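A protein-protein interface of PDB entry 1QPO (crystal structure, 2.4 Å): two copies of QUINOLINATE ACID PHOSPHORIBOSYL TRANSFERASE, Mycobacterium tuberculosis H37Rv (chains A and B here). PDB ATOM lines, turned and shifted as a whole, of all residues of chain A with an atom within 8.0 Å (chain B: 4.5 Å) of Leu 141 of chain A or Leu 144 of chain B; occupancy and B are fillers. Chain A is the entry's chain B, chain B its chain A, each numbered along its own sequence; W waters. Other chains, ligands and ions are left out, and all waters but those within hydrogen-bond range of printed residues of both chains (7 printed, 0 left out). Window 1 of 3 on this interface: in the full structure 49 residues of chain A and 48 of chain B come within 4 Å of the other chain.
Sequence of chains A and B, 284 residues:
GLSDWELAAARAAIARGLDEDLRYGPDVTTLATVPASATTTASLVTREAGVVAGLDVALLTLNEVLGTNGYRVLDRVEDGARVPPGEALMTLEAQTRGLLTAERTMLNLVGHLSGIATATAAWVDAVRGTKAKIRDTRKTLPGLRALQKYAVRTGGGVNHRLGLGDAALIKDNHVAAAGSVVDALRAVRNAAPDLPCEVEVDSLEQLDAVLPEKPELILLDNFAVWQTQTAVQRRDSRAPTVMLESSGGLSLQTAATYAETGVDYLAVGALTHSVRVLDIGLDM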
ATOM      1  N   ALA A  13      -6.925  -3.090   8.370  1.00  0.00           N
ATOM      2  CA  ALA A  13      -6.753  -4.339   7.624  1.00  0.00           C
ATOM      3  C   ALA A  13      -7.881  -5.302   7.935  1.00  0.00           C
ATOM      4  O   ALA A  13      -8.461  -5.850   7.009  1.00  0.00           O
ATOM      5  CB  ALA A  13      -5.420  -4.994   7.958  1.00  0.00           C
ATOM      6  N   ARG A  16     -10.983  -4.182   6.302  1.00  0.00           N
ATOM      7  CA  ARG A  16     -10.964  -4.503   4.864  1.00  0.00           C
ATOM      8  C   ARG A  16     -11.216  -5.991   4.597  1.00  0.00           C
ATOM      9  O   ARG A  16     -11.933  -6.361   3.647  1.00  0.00           O
ATOM     10  CB  ARG A  16      -9.643  -4.096   4.239  1.00  0.00           C
ATOM     11  CG  ARG A  16      -9.371  -2.614   4.315  1.00  0.00           C
ATOM     12  CD  ARG A  16      -8.138  -2.256   3.524  1.00  0.00           C
ATOM     13  NE  ARG A  16      -6.911  -2.386   4.296  1.00  0.00           N
ATOM     14  CZ  ARG A  16      -6.288  -1.357   4.868  1.00  0.00           C
ATOM     15  NH1 ARG A  16      -6.786  -0.118   4.769  1.00  0.00           N
ATOM     16  NH2 ARG A  16      -5.153  -1.566   5.517  1.00  0.00           N
ATOM     17  N   GLY A  17     -10.627  -6.858   5.418  1.00  0.00           N
ATOM     18  CA  GLY A  17     -10.852  -8.282   5.219  1.00  0.00           C
ATOM     19  C   GLY A  17     -12.316  -8.669   5.379  1.00  0.00           C
ATOM     20  O   GLY A  17     -12.864  -9.440   4.567  1.00  0.00           O
ATOM     21  N   GLU A  20     -14.494  -7.540   2.514  1.00  0.00           N
ATOM     22  CA  GLU A  20     -14.370  -8.386   1.350  1.00  0.00           C
ATOM     23  C   GLU A  20     -15.208  -9.617   1.515  1.00  0.00           C
ATOM     24  O   GLU A  20     -15.784 -10.137   0.547  1.00  0.00           O
ATOM     25  CB  GLU A  20     -12.939  -8.831   1.172  1.00  0.00           C
ATOM     26  CG  GLU A  20     -12.027  -7.712   0.769  1.00  0.00           C
ATOM     27  CD  GLU A  20     -10.570  -8.109   0.738  1.00  0.00           C
ATOM     28  OE1 GLU A  20     -10.105  -8.753   1.696  1.00  0.00           O
ATOM     29  OE2 GLU A  20      -9.893  -7.725  -0.241  1.00  0.00           O
ATOM     30  N   HIS A 112      -0.391 -15.162   8.180  1.00  0.00           N
ATOM     31  CA  HIS A 112       0.565 -14.386   7.421  1.00  0.00           C
ATOM     32  C   HIS A 112       1.623 -13.837   8.366  1.00  0.00           C
ATOM     33  O   HIS A 112       2.823 -14.020   8.148  1.00  0.00           O
ATOM     34  CB  HIS A 112      -0.148 -13.230   6.702  1.00  0.00           C
ATOM     35  CG  HIS A 112       0.752 -12.401   5.821  1.00  0.00           C
ATOM     36  ND1 HIS A 112       1.219 -12.841   4.597  1.00  0.00           N
ATOM     37  CD2 HIS A 112       1.272 -11.154   5.998  1.00  0.00           C
ATOM     38  CE1 HIS A 112       1.991 -11.908   4.065  1.00  0.00           C
ATOM     39  NE2 HIS A 112       2.039 -10.873   4.896  1.00  0.00           N
ATOM     40  N   ILE A 116       5.719 -14.595   8.658  1.00  0.00           N
ATOM     41  CA  ILE A 116       6.825 -13.654   8.636  1.00  0.00           C
ATOM     42  C   ILE A 116       7.753 -13.797   9.834  1.00  0.00           C
ATOM     43  O   ILE A 116       8.947 -13.875   9.678  1.00  0.00           O
ATOM     44  CB  ILE A 116       6.319 -12.221   8.621  1.00  0.00           C
ATOM     45  CG1 ILE A 116       5.540 -11.972   7.349  1.00  0.00           C
ATOM     46  CG2 ILE A 116       7.498 -11.271   8.671  1.00  0.00           C
ATOM     47  CD1 ILE A 116       4.987 -10.606   7.257  1.00  0.00           C
ATOM     48  N   THR A 137      12.824  -4.504   4.799  1.00  0.00           N
ATOM     49  CA  THR A 137      12.884  -3.522   3.746  1.00  0.00           C
ATOM     50  C   THR A 137      11.515  -2.820   3.500  1.00  0.00           C
ATOM     51  O   THR A 137      10.591  -2.935   4.292  1.00  0.00           O
ATOM     52  CB  THR A 137      13.347  -4.252   2.442  1.00  0.00           C
ATOM     53  OG1 THR A 137      12.295  -5.082   1.970  1.00  0.00           O
ATOM     54  CG2 THR A 137      14.562  -5.144   2.682  1.00  0.00           C
ATOM     55  N   ARG A 138      11.444  -2.019   2.442  1.00  0.00           N
ATOM     56  CA  ARG A 138      10.205  -1.353   2.015  1.00  0.00           C
ATOM     57  C   ARG A 138       9.493  -2.238   0.973  1.00  0.00           C
ATOM     58  O   ARG A 138       8.521  -1.804   0.356  1.00  0.00           O
ATOM     59  CB  ARG A 138      10.466   0.030   1.410  1.00  0.00           C
ATOM     60  CG  ARG A 138      10.810   1.124   2.432  1.00  0.00           C
ATOM     61  CD  ARG A 138      10.568   2.513   1.852  1.00  0.00           C
ATOM     62  NE  ARG A 138      11.386   2.715   0.673  1.00  0.00           N
ATOM     63  CZ  ARG A 138      10.919   3.029  -0.520  1.00  0.00           C
ATOM     64  NH1 ARG A 138       9.638   3.189  -0.701  1.00  0.00           N
ATOM     65  NH2 ARG A 138      11.738   3.118  -1.555  1.00  0.00           N
ATOM     66  N   LYS A 139      10.003  -3.456   0.747  1.00  0.00           N
ATOM     67  CA  LYS A 139       9.356  -4.402  -0.161  1.00  0.00           C
ATOM     68  C   LYS A 139       8.224  -5.097   0.632  1.00  0.00           C
ATOM     69  O   LYS A 139       8.294  -6.285   0.924  1.00  0.00           O
ATOM     70  CB  LYS A 139      10.349  -5.441  -0.636  1.00  0.00           C
ATOM     71  CG  LYS A 139      11.568  -4.831  -1.205  1.00  0.00           C
ATOM     72  CD  LYS A 139      12.316  -5.852  -1.971  1.00  0.00           C
ATOM     73  CE  LYS A 139      13.598  -5.251  -2.460  1.00  0.00           C
ATOM     74  NZ  LYS A 139      14.116  -6.097  -3.567  1.00  0.00           N
ATOM     75  N   THR A 140       7.205  -4.322   1.000  1.00  0.00           N
ATOM     76  CA  THR A 140       6.059  -4.786   1.776  1.00  0.00           C
ATOM     77  C   THR A 140       4.799  -4.809   0.915  1.00  0.00           C
ATOM     78  O   THR A 140       4.808  -4.308  -0.210  1.00  0.00           O
ATOM     79  CB  THR A 140       5.863  -3.870   2.990  1.00  0.00           C
ATOM     80  OG1 THR A 140       5.931  -2.502   2.573  1.00  0.00           O
ATOM     81  CG2 THR A 140       6.976  -4.094   4.004  1.00  0.00           C
ATOM     82  N   LEU A 141       3.724  -5.436   1.389  1.00  0.00           N
ATOM     83  CA  LEU A 141       2.477  -5.460   0.614  1.00  0.00           C
ATOM     84  C   LEU A 141       1.696  -4.200   0.959  1.00  0.00           C
ATOM     85  O   LEU A 141       1.568  -3.863   2.124  1.00  0.00           O
ATOM     86  CB  LEU A 141       1.656  -6.692   0.948  1.00  0.00           C
ATOM     87  CG  LEU A 141       1.706  -7.915   0.041  1.00  0.00           C
ATOM     88  CD1 LEU A 141       2.390  -7.550  -1.273  1.00  0.00           C
ATOM     89  CD2 LEU A 141       2.398  -9.084   0.737  1.00  0.00           C
ATOM     90  N   PRO A 142       1.186  -3.479  -0.049  1.00  0.00           N
ATOM     91  CA  PRO A 142       0.421  -2.237   0.141  1.00  0.00           C
ATOM     92  C   PRO A 142      -0.702  -2.350   1.124  1.00  0.00           C
ATOM     93  O   PRO A 142      -1.625  -3.143   0.937  1.00  0.00           O
ATOM     94  CB  PRO A 142      -0.094  -1.931  -1.262  1.00  0.00           C
ATOM     95  CG  PRO A 142      -0.020  -3.238  -1.977  1.00  0.00           C
ATOM     96  CD  PRO A 142       1.242  -3.833  -1.477  1.00  0.00           C
ATOM     97  N   GLY A 143      -0.602  -1.579   2.200  1.00  0.00           N
ATOM     98  CA  GLY A 143      -1.647  -1.585   3.201  1.00  0.00           C
ATOM     99  C   GLY A 143      -1.311  -2.464   4.365  1.00  0.00           C
ATOM    100  O   GLY A 143      -1.946  -2.350   5.401  1.00  0.00           O
ATOM    101  N   LEU A 144      -0.240  -3.252   4.248  1.00  0.00           N
ATOM    102  CA  LEU A 144       0.148  -4.163   5.320  1.00  0.00           C
ATOM    103  C   LEU A 144       1.514  -3.877   5.894  1.00  0.00           C
ATOM    104  O   LEU A 144       1.997  -4.642   6.746  1.00  0.00           O
ATOM    105  CB  LEU A 144       0.104  -5.612   4.836  1.00  0.00           C
ATOM    106  CG  LEU A 144      -1.234  -6.214   4.377  1.00  0.00           C
ATOM    107  CD1 LEU A 144      -1.003  -7.625   3.858  1.00  0.00           C
ATOM    108  CD2 LEU A 144      -2.231  -6.265   5.511  1.00  0.00           C
ATOM    109  N   ARG A 145       2.122  -2.760   5.510  1.00  0.00           N
ATOM    110  CA  ARG A 145       3.447  -2.439   6.034  1.00  0.00           C
ATOM    111  C   ARG A 145       3.615  -2.405   7.522  1.00  0.00           C
ATOM    112  O   ARG A 145       4.541  -3.023   8.014  1.00  0.00           O
ATOM    113  CB  ARG A 145       4.044  -1.161   5.432  1.00  0.00           C
ATOM    114  CG  ARG A 145       5.407  -0.764   6.050  1.00  0.00           C
ATOM    115  CD  ARG A 145       6.071   0.360   5.276  1.00  0.00           C
ATOM    116  NE  ARG A 145       6.343  -0.034   3.901  1.00  0.00           N
ATOM    117  CZ  ARG A 145       6.636   0.809   2.918  1.00  0.00           C
ATOM    118  NH1 ARG A 145       6.698   2.119   3.146  1.00  0.00           N
ATOM    119  NH2 ARG A 145       6.878   0.322   1.702  1.00  0.00           N
ATOM    120  N   ALA A 146       2.767  -1.693   8.260  1.00  0.00           N
ATOM    121  CA  ALA A 146       2.928  -1.630   9.720  1.00  0.00           C
ATOM    122  C   ALA A 146       2.863  -3.014  10.352  1.00  0.00           C
ATOM    123  O   ALA A 146       3.641  -3.327  11.254  1.00  0.00           O
ATOM    124  CB  ALA A 146       1.893  -0.743  10.332  1.00  0.00           C
ATOM    125  N   LEU A 147       1.972  -3.858   9.840  1.00  0.00           N
ATOM    126  CA  LEU A 147       1.805  -5.212  10.356  1.00  0.00           C
ATOM    127  C   LEU A 147       2.989  -6.114   9.992  1.00  0.00           C
ATOM    128  O   LEU A 147       3.495  -6.846  10.821  1.00  0.00           O
ATOM    129  CB  LEU A 147       0.487  -5.804   9.844  1.00  0.00           C
ATOM    130  CG  LEU A 147      -0.775  -5.123  10.400  1.00  0.00           C
ATOM    131  CD1 LEU A 147      -1.967  -5.924   9.977  1.00  0.00           C
ATOM    132  CD2 LEU A 147      -0.735  -5.035  11.933  1.00  0.00           C
ATOM    133  N   GLN A 148       3.441  -6.041   8.752  1.00  0.00           N
ATOM    134  CA  GLN A 148       4.558  -6.840   8.347  1.00  0.00           C
ATOM    135  C   GLN A 148       5.810  -6.471   9.124  1.00  0.00           C
ATOM    136  O   GLN A 148       6.580  -7.313   9.528  1.00  0.00           O
ATOM    137  CB  GLN A 148       4.768  -6.682   6.865  1.00  0.00           C
ATOM    138  CG  GLN A 148       3.650  -7.299   6.051  1.00  0.00           C
ATOM    139  CD  GLN A 148       4.017  -7.382   4.598  1.00  0.00           C
ATOM    140  OE1 GLN A 148       3.897  -8.432   3.963  1.00  0.00           O
ATOM    141  NE2 GLN A 148       4.504  -6.286   4.069  1.00  0.00           N
ATOM    142  N   THR A 272       9.284 -10.094   3.840  1.00  0.00           N
ATOM    143  CA  THR A 272       8.012  -9.417   3.589  1.00  0.00           C
ATOM    144  C   THR A 272       7.373  -9.651   2.244  1.00  0.00           C
ATOM    145  O   THR A 272       6.162  -9.529   2.107  1.00  0.00           O
ATOM    146  CB  THR A 272       8.140  -7.940   3.841  1.00  0.00           C
ATOM    147  OG1 THR A 272       9.252  -7.443   3.104  1.00  0.00           O
ATOM    148  CG2 THR A 272       8.391  -7.692   5.326  1.00  0.00           C
ATOM    149  N   HIS A 273       8.171  -9.821   1.201  1.00  0.00           N
ATOM    150  CA  HIS A 273       7.565 -10.212  -0.087  1.00  0.00           C
ATOM    151  C   HIS A 273       7.786 -11.731   0.005  1.00  0.00           C
ATOM    152  O   HIS A 273       8.472 -12.173   0.921  1.00  0.00           O
ATOM    153  CB  HIS A 273       8.266  -9.558  -1.297  1.00  0.00           C
ATOM    154  CG  HIS A 273       9.704  -9.946  -1.494  1.00  0.00           C
ATOM    155  ND1 HIS A 273      10.106 -11.244  -1.736  1.00  0.00           N
ATOM    156  CD2 HIS A 273      10.822  -9.183  -1.572  1.00  0.00           C
ATOM    157  CE1 HIS A 273      11.405 -11.263  -1.956  1.00  0.00           C
ATOM    158  NE2 HIS A 273      11.861 -10.025  -1.867  1.00  0.00           N
ATOM    159  N   SER A 274       7.223 -12.579  -0.826  1.00  0.00           N
ATOM    160  CA  SER A 274       7.567 -14.011  -0.571  1.00  0.00           C
ATOM    161  C   SER A 274       7.339 -14.604   0.853  1.00  0.00           C
ATOM    162  O   SER A 274       8.214 -15.271   1.374  1.00  0.00           O
ATOM    163  CB  SER A 274       9.043 -14.307  -0.955  1.00  0.00           C
ATOM    164  OG  SER A 274       9.341 -13.865  -2.283  1.00  0.00           O
ATOM    165  N   VAL A 275       6.198 -14.404   1.505  1.00  0.00           N
ATOM    166  CA  VAL A 275       6.048 -15.033   2.821  1.00  0.00           C
ATOM    167  C   VAL A 275       5.180 -16.303   2.731  1.00  0.00           C
ATOM    168  O   VAL A 275       4.272 -16.369   1.905  1.00  0.00           O
ATOM    169  CB  VAL A 275       5.560 -14.069   3.942  1.00  0.00           C
ATOM    170  CG1 VAL A 275       5.491 -12.647   3.467  1.00  0.00           C
ATOM    171  CG2 VAL A 275       4.254 -14.535   4.510  1.00  0.00           C
ATOM    172  N   ALA B  13      -5.705  -0.070  -3.314  1.00  0.00           N
ATOM    173  CA  ALA B  13      -4.431  -0.628  -2.882  1.00  0.00           C
ATOM    174  C   ALA B  13      -3.281   0.351  -3.186  1.00  0.00           C
ATOM    175  O   ALA B  13      -2.497   0.672  -2.276  1.00  0.00           O
ATOM    176  CB  ALA B  13      -4.181  -1.932  -3.558  1.00  0.00           C
ATOM    177  N   GLU B  20       1.605   4.865   2.789  1.00  0.00           N
ATOM    178  CA  GLU B  20       2.587   4.294   3.686  1.00  0.00           C
ATOM    179  C   GLU B  20       3.953   4.890   3.332  1.00  0.00           C
ATOM    180  O   GLU B  20       4.720   5.304   4.212  1.00  0.00           O
ATOM    181  CB  GLU B  20       2.650   2.790   3.489  1.00  0.00           C
ATOM    182  CG  GLU B  20       1.379   2.075   3.852  1.00  0.00           C
ATOM    183  CD  GLU B  20       1.442   0.573   3.594  1.00  0.00           C
ATOM    184  OE1 GLU B  20       1.838   0.171   2.473  1.00  0.00           O
ATOM    185  OE2 GLU B  20       1.069  -0.199   4.506  1.00  0.00           O
ATOM    186  N   ASN B 108       6.290  -3.441  -5.848  1.00  0.00           N
ATOM    187  CA  ASN B 108       5.741  -4.311  -4.814  1.00  0.00           C
ATOM    188  C   ASN B 108       4.445  -4.938  -5.305  1.00  0.00           C
ATOM    189  O   ASN B 108       4.196  -6.119  -5.080  1.00  0.00           O
ATOM    190  CB  ASN B 108       5.432  -3.526  -3.546  1.00  0.00           C
ATOM    191  CG  ASN B 108       6.656  -3.162  -2.786  1.00  0.00           C
ATOM    192  OD1 ASN B 108       7.702  -3.728  -3.012  1.00  0.00           O
ATOM    193  ND2 ASN B 108       6.542  -2.218  -1.863  1.00  0.00           N
ATOM    194  N   HIS B 112       4.120  -8.907  -6.769  1.00  0.00           N
ATOM    195  CA  HIS B 112       3.249  -9.808  -6.024  1.00  0.00           C
ATOM    196  C   HIS B 112       2.265 -10.488  -6.962  1.00  0.00           C
ATOM    197  O   HIS B 112       2.103 -11.719  -6.961  1.00  0.00           O
ATOM    198  CB  HIS B 112       2.478  -9.031  -4.963  1.00  0.00           C
ATOM    199  CG  HIS B 112       1.625  -9.894  -4.076  1.00  0.00           C
ATOM    200  ND1 HIS B 112       2.135 -10.607  -3.012  1.00  0.00           N
ATOM    201  CD2 HIS B 112       0.292 -10.154  -4.096  1.00  0.00           C
ATOM    202  CE1 HIS B 112       1.158 -11.275  -2.421  1.00  0.00           C
ATOM    203  NE2 HIS B 112       0.033 -11.019  -3.062  1.00  0.00           N
ATOM    204  N   LEU B 141      -5.079 -12.111   1.153  1.00  0.00           N
ATOM    205  CA  LEU B 141      -4.618 -11.161   2.143  1.00  0.00           C
ATOM    206  C   LEU B 141      -5.636 -10.062   2.217  1.00  0.00           C
ATOM    207  O   LEU B 141      -6.089  -9.589   1.196  1.00  0.00           O
ATOM    208  CB  LEU B 141      -3.271 -10.559   1.751  1.00  0.00           C
ATOM    209  CG  LEU B 141      -1.944 -11.069   2.289  1.00  0.00           C
ATOM    210  CD1 LEU B 141      -2.211 -11.846   3.602  1.00  0.00           C
ATOM    211  CD2 LEU B 141      -1.241 -11.920   1.214  1.00  0.00           C
ATOM    212  N   PRO B 142      -5.982  -9.621   3.432  1.00  0.00           N
ATOM    213  CA  PRO B 142      -6.957  -8.553   3.668  1.00  0.00           C
ATOM    214  C   PRO B 142      -6.674  -7.311   2.850  1.00  0.00           C
ATOM    215  O   PRO B 142      -5.585  -6.751   2.893  1.00  0.00           O
ATOM    216  CB  PRO B 142      -6.830  -8.271   5.184  1.00  0.00           C
ATOM    217  CG  PRO B 142      -5.485  -8.829   5.548  1.00  0.00           C
ATOM    218  CD  PRO B 142      -5.414 -10.090   4.709  1.00  0.00           C
ATOM    219  N   GLY B 143      -7.668  -6.895   2.088  1.00  0.00           N
ATOM    220  CA  GLY B 143      -7.489  -5.734   1.274  1.00  0.00           C
ATOM    221  C   GLY B 143      -6.995  -6.067  -0.108  1.00  0.00           C
ATOM    222  O   GLY B 143      -7.126  -5.224  -0.989  1.00  0.00           O
ATOM    223  N   LEU B 144      -6.497  -7.288  -0.334  1.00  0.00           N
ATOM    224  CA  LEU B 144      -5.961  -7.653  -1.647  1.00  0.00           C
ATOM    225  C   LEU B 144      -6.679  -8.754  -2.414  1.00  0.00           C
ATOM    226  O   LEU B 144      -6.210  -9.168  -3.486  1.00  0.00           O
ATOM    227  CB  LEU B 144      -4.479  -8.012  -1.533  1.00  0.00           C
ATOM    228  CG  LEU B 144      -3.504  -6.930  -1.081  1.00  0.00           C
ATOM    229  CD1 LEU B 144      -2.141  -7.527  -0.850  1.00  0.00           C
ATOM    230  CD2 LEU B 144      -3.409  -5.860  -2.126  1.00  0.00           C
ATOM    231  N   ARG B 145      -7.851  -9.182  -1.951  1.00  0.00           N
ATOM    232  CA  ARG B 145      -8.573 -10.250  -2.643  1.00  0.00           C
ATOM    233  C   ARG B 145      -8.892 -10.129  -4.152  1.00  0.00           C
ATOM    234  O   ARG B 145      -8.575 -11.048  -4.926  1.00  0.00           O
ATOM    235  CB  ARG B 145      -9.813 -10.659  -1.877  1.00  0.00           C
ATOM    236  CG  ARG B 145     -10.595 -11.718  -2.615  1.00  0.00           C
ATOM    237  CD  ARG B 145     -11.697 -12.259  -1.757  1.00  0.00           C
ATOM    238  NE  ARG B 145     -11.173 -12.845  -0.548  1.00  0.00           N
ATOM    239  CZ  ARG B 145     -11.924 -13.101   0.515  1.00  0.00           C
ATOM    240  NH1 ARG B 145     -13.227 -12.817   0.490  1.00  0.00           N
ATOM    241  NH2 ARG B 145     -11.370 -13.612   1.621  1.00  0.00           N
ATOM    242  N   ALA B 146      -9.517  -9.028  -4.578  1.00  0.00           N
ATOM    243  CA  ALA B 146      -9.860  -8.857  -5.976  1.00  0.00           C
ATOM    244  C   ALA B 146      -8.635  -8.951  -6.845  1.00  0.00           C
ATOM    245  O   ALA B 146      -8.667  -9.616  -7.884  1.00  0.00           O
ATOM    246  CB  ALA B 146     -10.579  -7.505  -6.204  1.00  0.00           C
ATOM    247  N   LEU B 147      -7.547  -8.329  -6.396  1.00  0.00           N
ATOM    248  CA  LEU B 147      -6.286  -8.314  -7.145  1.00  0.00           C
ATOM    249  C   LEU B 147      -5.655  -9.712  -7.195  1.00  0.00           C
ATOM    250  O   LEU B 147      -5.254 -10.190  -8.257  1.00  0.00           O
ATOM    251  CB  LEU B 147      -5.314  -7.257  -6.544  1.00  0.00           C
ATOM    252  CG  LEU B 147      -5.676  -5.770  -6.726  1.00  0.00           C
ATOM    253  CD1 LEU B 147      -4.489  -4.888  -6.382  1.00  0.00           C
ATOM    254  CD2 LEU B 147      -6.049  -5.482  -8.175  1.00  0.00           C
ATOM    255  N   GLN B 148      -5.624 -10.397  -6.056  1.00  0.00           N
ATOM    256  CA  GLN B 148      -5.047 -11.738  -6.028  1.00  0.00           C
ATOM    257  C   GLN B 148      -5.907 -12.669  -6.852  1.00  0.00           C
ATOM    258  O   GLN B 148      -5.398 -13.527  -7.536  1.00  0.00           O
ATOM    259  CB  GLN B 148      -4.930 -12.258  -4.601  1.00  0.00           C
ATOM    260  CG  GLN B 148      -4.001 -11.439  -3.753  1.00  0.00           C
ATOM    261  CD  GLN B 148      -3.741 -12.090  -2.437  1.00  0.00           C
ATOM    262  OE1 GLN B 148      -2.611 -12.259  -2.038  1.00  0.00           O
ATOM    263  NE2 GLN B 148      -4.773 -12.489  -1.770  1.00  0.00           N
HETATM  264  O   HOH W   1      -8.461 -10.905   1.845  1.00  0.00           O
HETATM  265  O   HOH W   2      -4.859  -4.000   4.205  1.00  0.00           O
HETATM  266  O   HOH W   3       5.195 -10.793  -2.641  1.00  0.00           O
HETATM  267  O   HOH W   4       3.941  -1.593  -0.967  1.00  0.00           O
HETATM  268  O   HOH W   5       0.311  -0.273   7.050  1.00  0.00           O
HETATM  269  O   HOH W   6       3.859  -1.525   1.748  1.00  0.00           O
HETATM  270  O   HOH W   7      -4.204  -3.867   1.521  1.00  0.00           O
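CB of Pro 142 of chain B touches O of Ala 13 of chain A (3.4 Å).
Pro 142 of chain B touches Glu 20 of chain A.
His 112 of chain A touches Leu 141 of chain B.
Lys 139 of chain A touches Asn 108 of chain B (CA to OD1, 3.4 Å).
CD1 of Leu 141 of chain A touches ND1 of His 112 of chain B, 3.5 Å away.
Leu 144 of chain B touches Leu 141 of chain A.
Ala 13 of chain B touches Pro 142 of chain A.
Pro 142 of chain A touches Glu 20 of chain B.
Leu 141 of chain B touches Leu 144 of chain A.
The backbone carbonyl oxygen (O) of Arg 138 of chain A sits at hydrogen-bond distance from the side-chain hydroxyl (OG1) of Thr 140 of chain A.
The guanidinium group (NH2) of Arg 145 of chain A lies within hydrogen-bond range of the backbone carbonyl oxygen (O) of Arg 138 of chain A, at 3.0 Å.
A ring nitrogen (NE2) of His 112 of chain A lies within hydrogen-bond range of the side-chain amide oxygen of Gln 148 of chain A.
The backbone NH (N) of Leu 141 of chain A lies close to the side-chain amide nitrogen (NE2) of Gln 148 of chain A (2.9 Å).
NE2 of His 112 of chain B sits at hydrogen-bond distance from OE1 of Gln 148 of chain B, 3.1 Å away.
O of Lys 139 of chain A is in hydrogen-bond range of OG1 of Thr 272 of chain A (2.6 Å).
The side-chain carboxylate of Glu 20 of chain B lies within hydrogen-bond range of the backbone NH of Leu 144 of chain A, 3.3 Å away.
The backbone carbonyl oxygen of Thr 140 of chain A lies within hydrogen-bond range of the side-chain amide nitrogen of Asn 108 of chain B (3.2 Å).
OE2 of Glu 20 of chain A lies within hydrogen-bond range of N of Leu 144 of chain B (3.4 Å).
OE1 of Glu 20 of chain A sits at hydrogen-bond distance from N of Gly 143 of chain B (3.1 Å).
The side-chain carboxylate (OE1) of Glu 20 of chain B is in hydrogen-bond range of the backbone NH (N) of Gly 143 of chain A (3.0 Å).
The side-chain carboxylate (OE2) of Glu 20 of chain B sits at hydrogen-bond distance from the backbone NH (N) of Arg 145 of chain A, 2.9 Å away.
The side-chain carboxylate of Glu 20 of chain A is in hydrogen-bond range of the backbone NH of Arg 145 of chain B (3.0 Å).
ND2 of Asn 108 of chain B is in hydrogen-bond range of O of Arg 138 of chain A (3.0 Å).
Water W6 lies within hydrogen-bond range of OG1 of Thr 140 of chain A (2.4 Å), OE1 of Glu 20 of chain B (2.7 Å) and O of Leu 141 of chain A (3.3 Å).
Water W2 lies within hydrogen-bond range of NE of Arg 16 of chain A (2.6 Å) and O of Pro 142 of chain B (3.1 Å).
Water W5 lies within hydrogen-bond range of OE2 of Glu 20 of chain B (2.7 Å), N of Ala 146 of chain A (3.1 Å), N of Arg 145 of chain A (3.4 Å) and O of Gly 143 of chain A (3.5 Å).
Water W1 bridges OE1 of Glu 20 of chain A (2.7 Å) and O of Leu 141 of chain B (2.8 Å).
Water W7 bridges O of Pro 142 of chain A and O of Pro 142 of chain B.
Water W4 lies within hydrogen-bond range of ND2 of Asn 108 of chain B (2.8 Å) and O of Thr 140 of chain A (2.9 Å).
Of the printed residues of chain B, Ala 13 of chain A touches Pro 142 (3.4 Å).
Of the printed residues of chain B, Lys 139 of chain A touches Asn 108 (3.4 Å).
Leu 141 of chain A touches just these residues of chain B: His 112 and Leu 144.
Leu 144 of chain B touches two residues of chain A.
The nearest residue of chain A that does not touch Leu 144 of chain B is Pro 142 of chain A (4.3 Å).
Printed residues of chain A that touch a printed residue of chain B: Ala 13, Glu 20, His 112, Arg 138, Lys 139, Thr 140, Leu 141, Pro 142, Gly 143, Leu 144 and Arg 145.
Hydrophobic or aromatic side chains of chain A within 4 Å of the printed part of chain B: His 112, Leu 141, Pro 142 and Leu 144.
Among the printed residues, no Asp or Glu carboxylate lies within 4 Å of a Lys or Arg side-chain nitrogen of the other chain.
Glu 20 of chain A touches Pro 142 of chain B, and with the chains exchanged Pro 142 of chain A touches Glu 20 of chain B.
Glu 20 of chain A touches Gly 143 of chain B, and with the chains exchanged Gly 143 of chain A touches Glu 20 of chain B.
Glu 20 of chain A touches Leu 144 of chain B, and with the chains exchanged Leu 144 of chain A touches Glu 20 of chain B.
Leu 141 of chain A touches Leu 144 of chain B, and with the chains exchanged Leu 144 of chain A touches Leu 141 of chain B.
Positions printed for both chains: 13, 20, 112, 141, 142, 143, 144, 145, 146, 147 and 148.
Of the 17 pairs that touch across the chains among the printed residues, 14 have their exchanged pair printed and touching as well.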
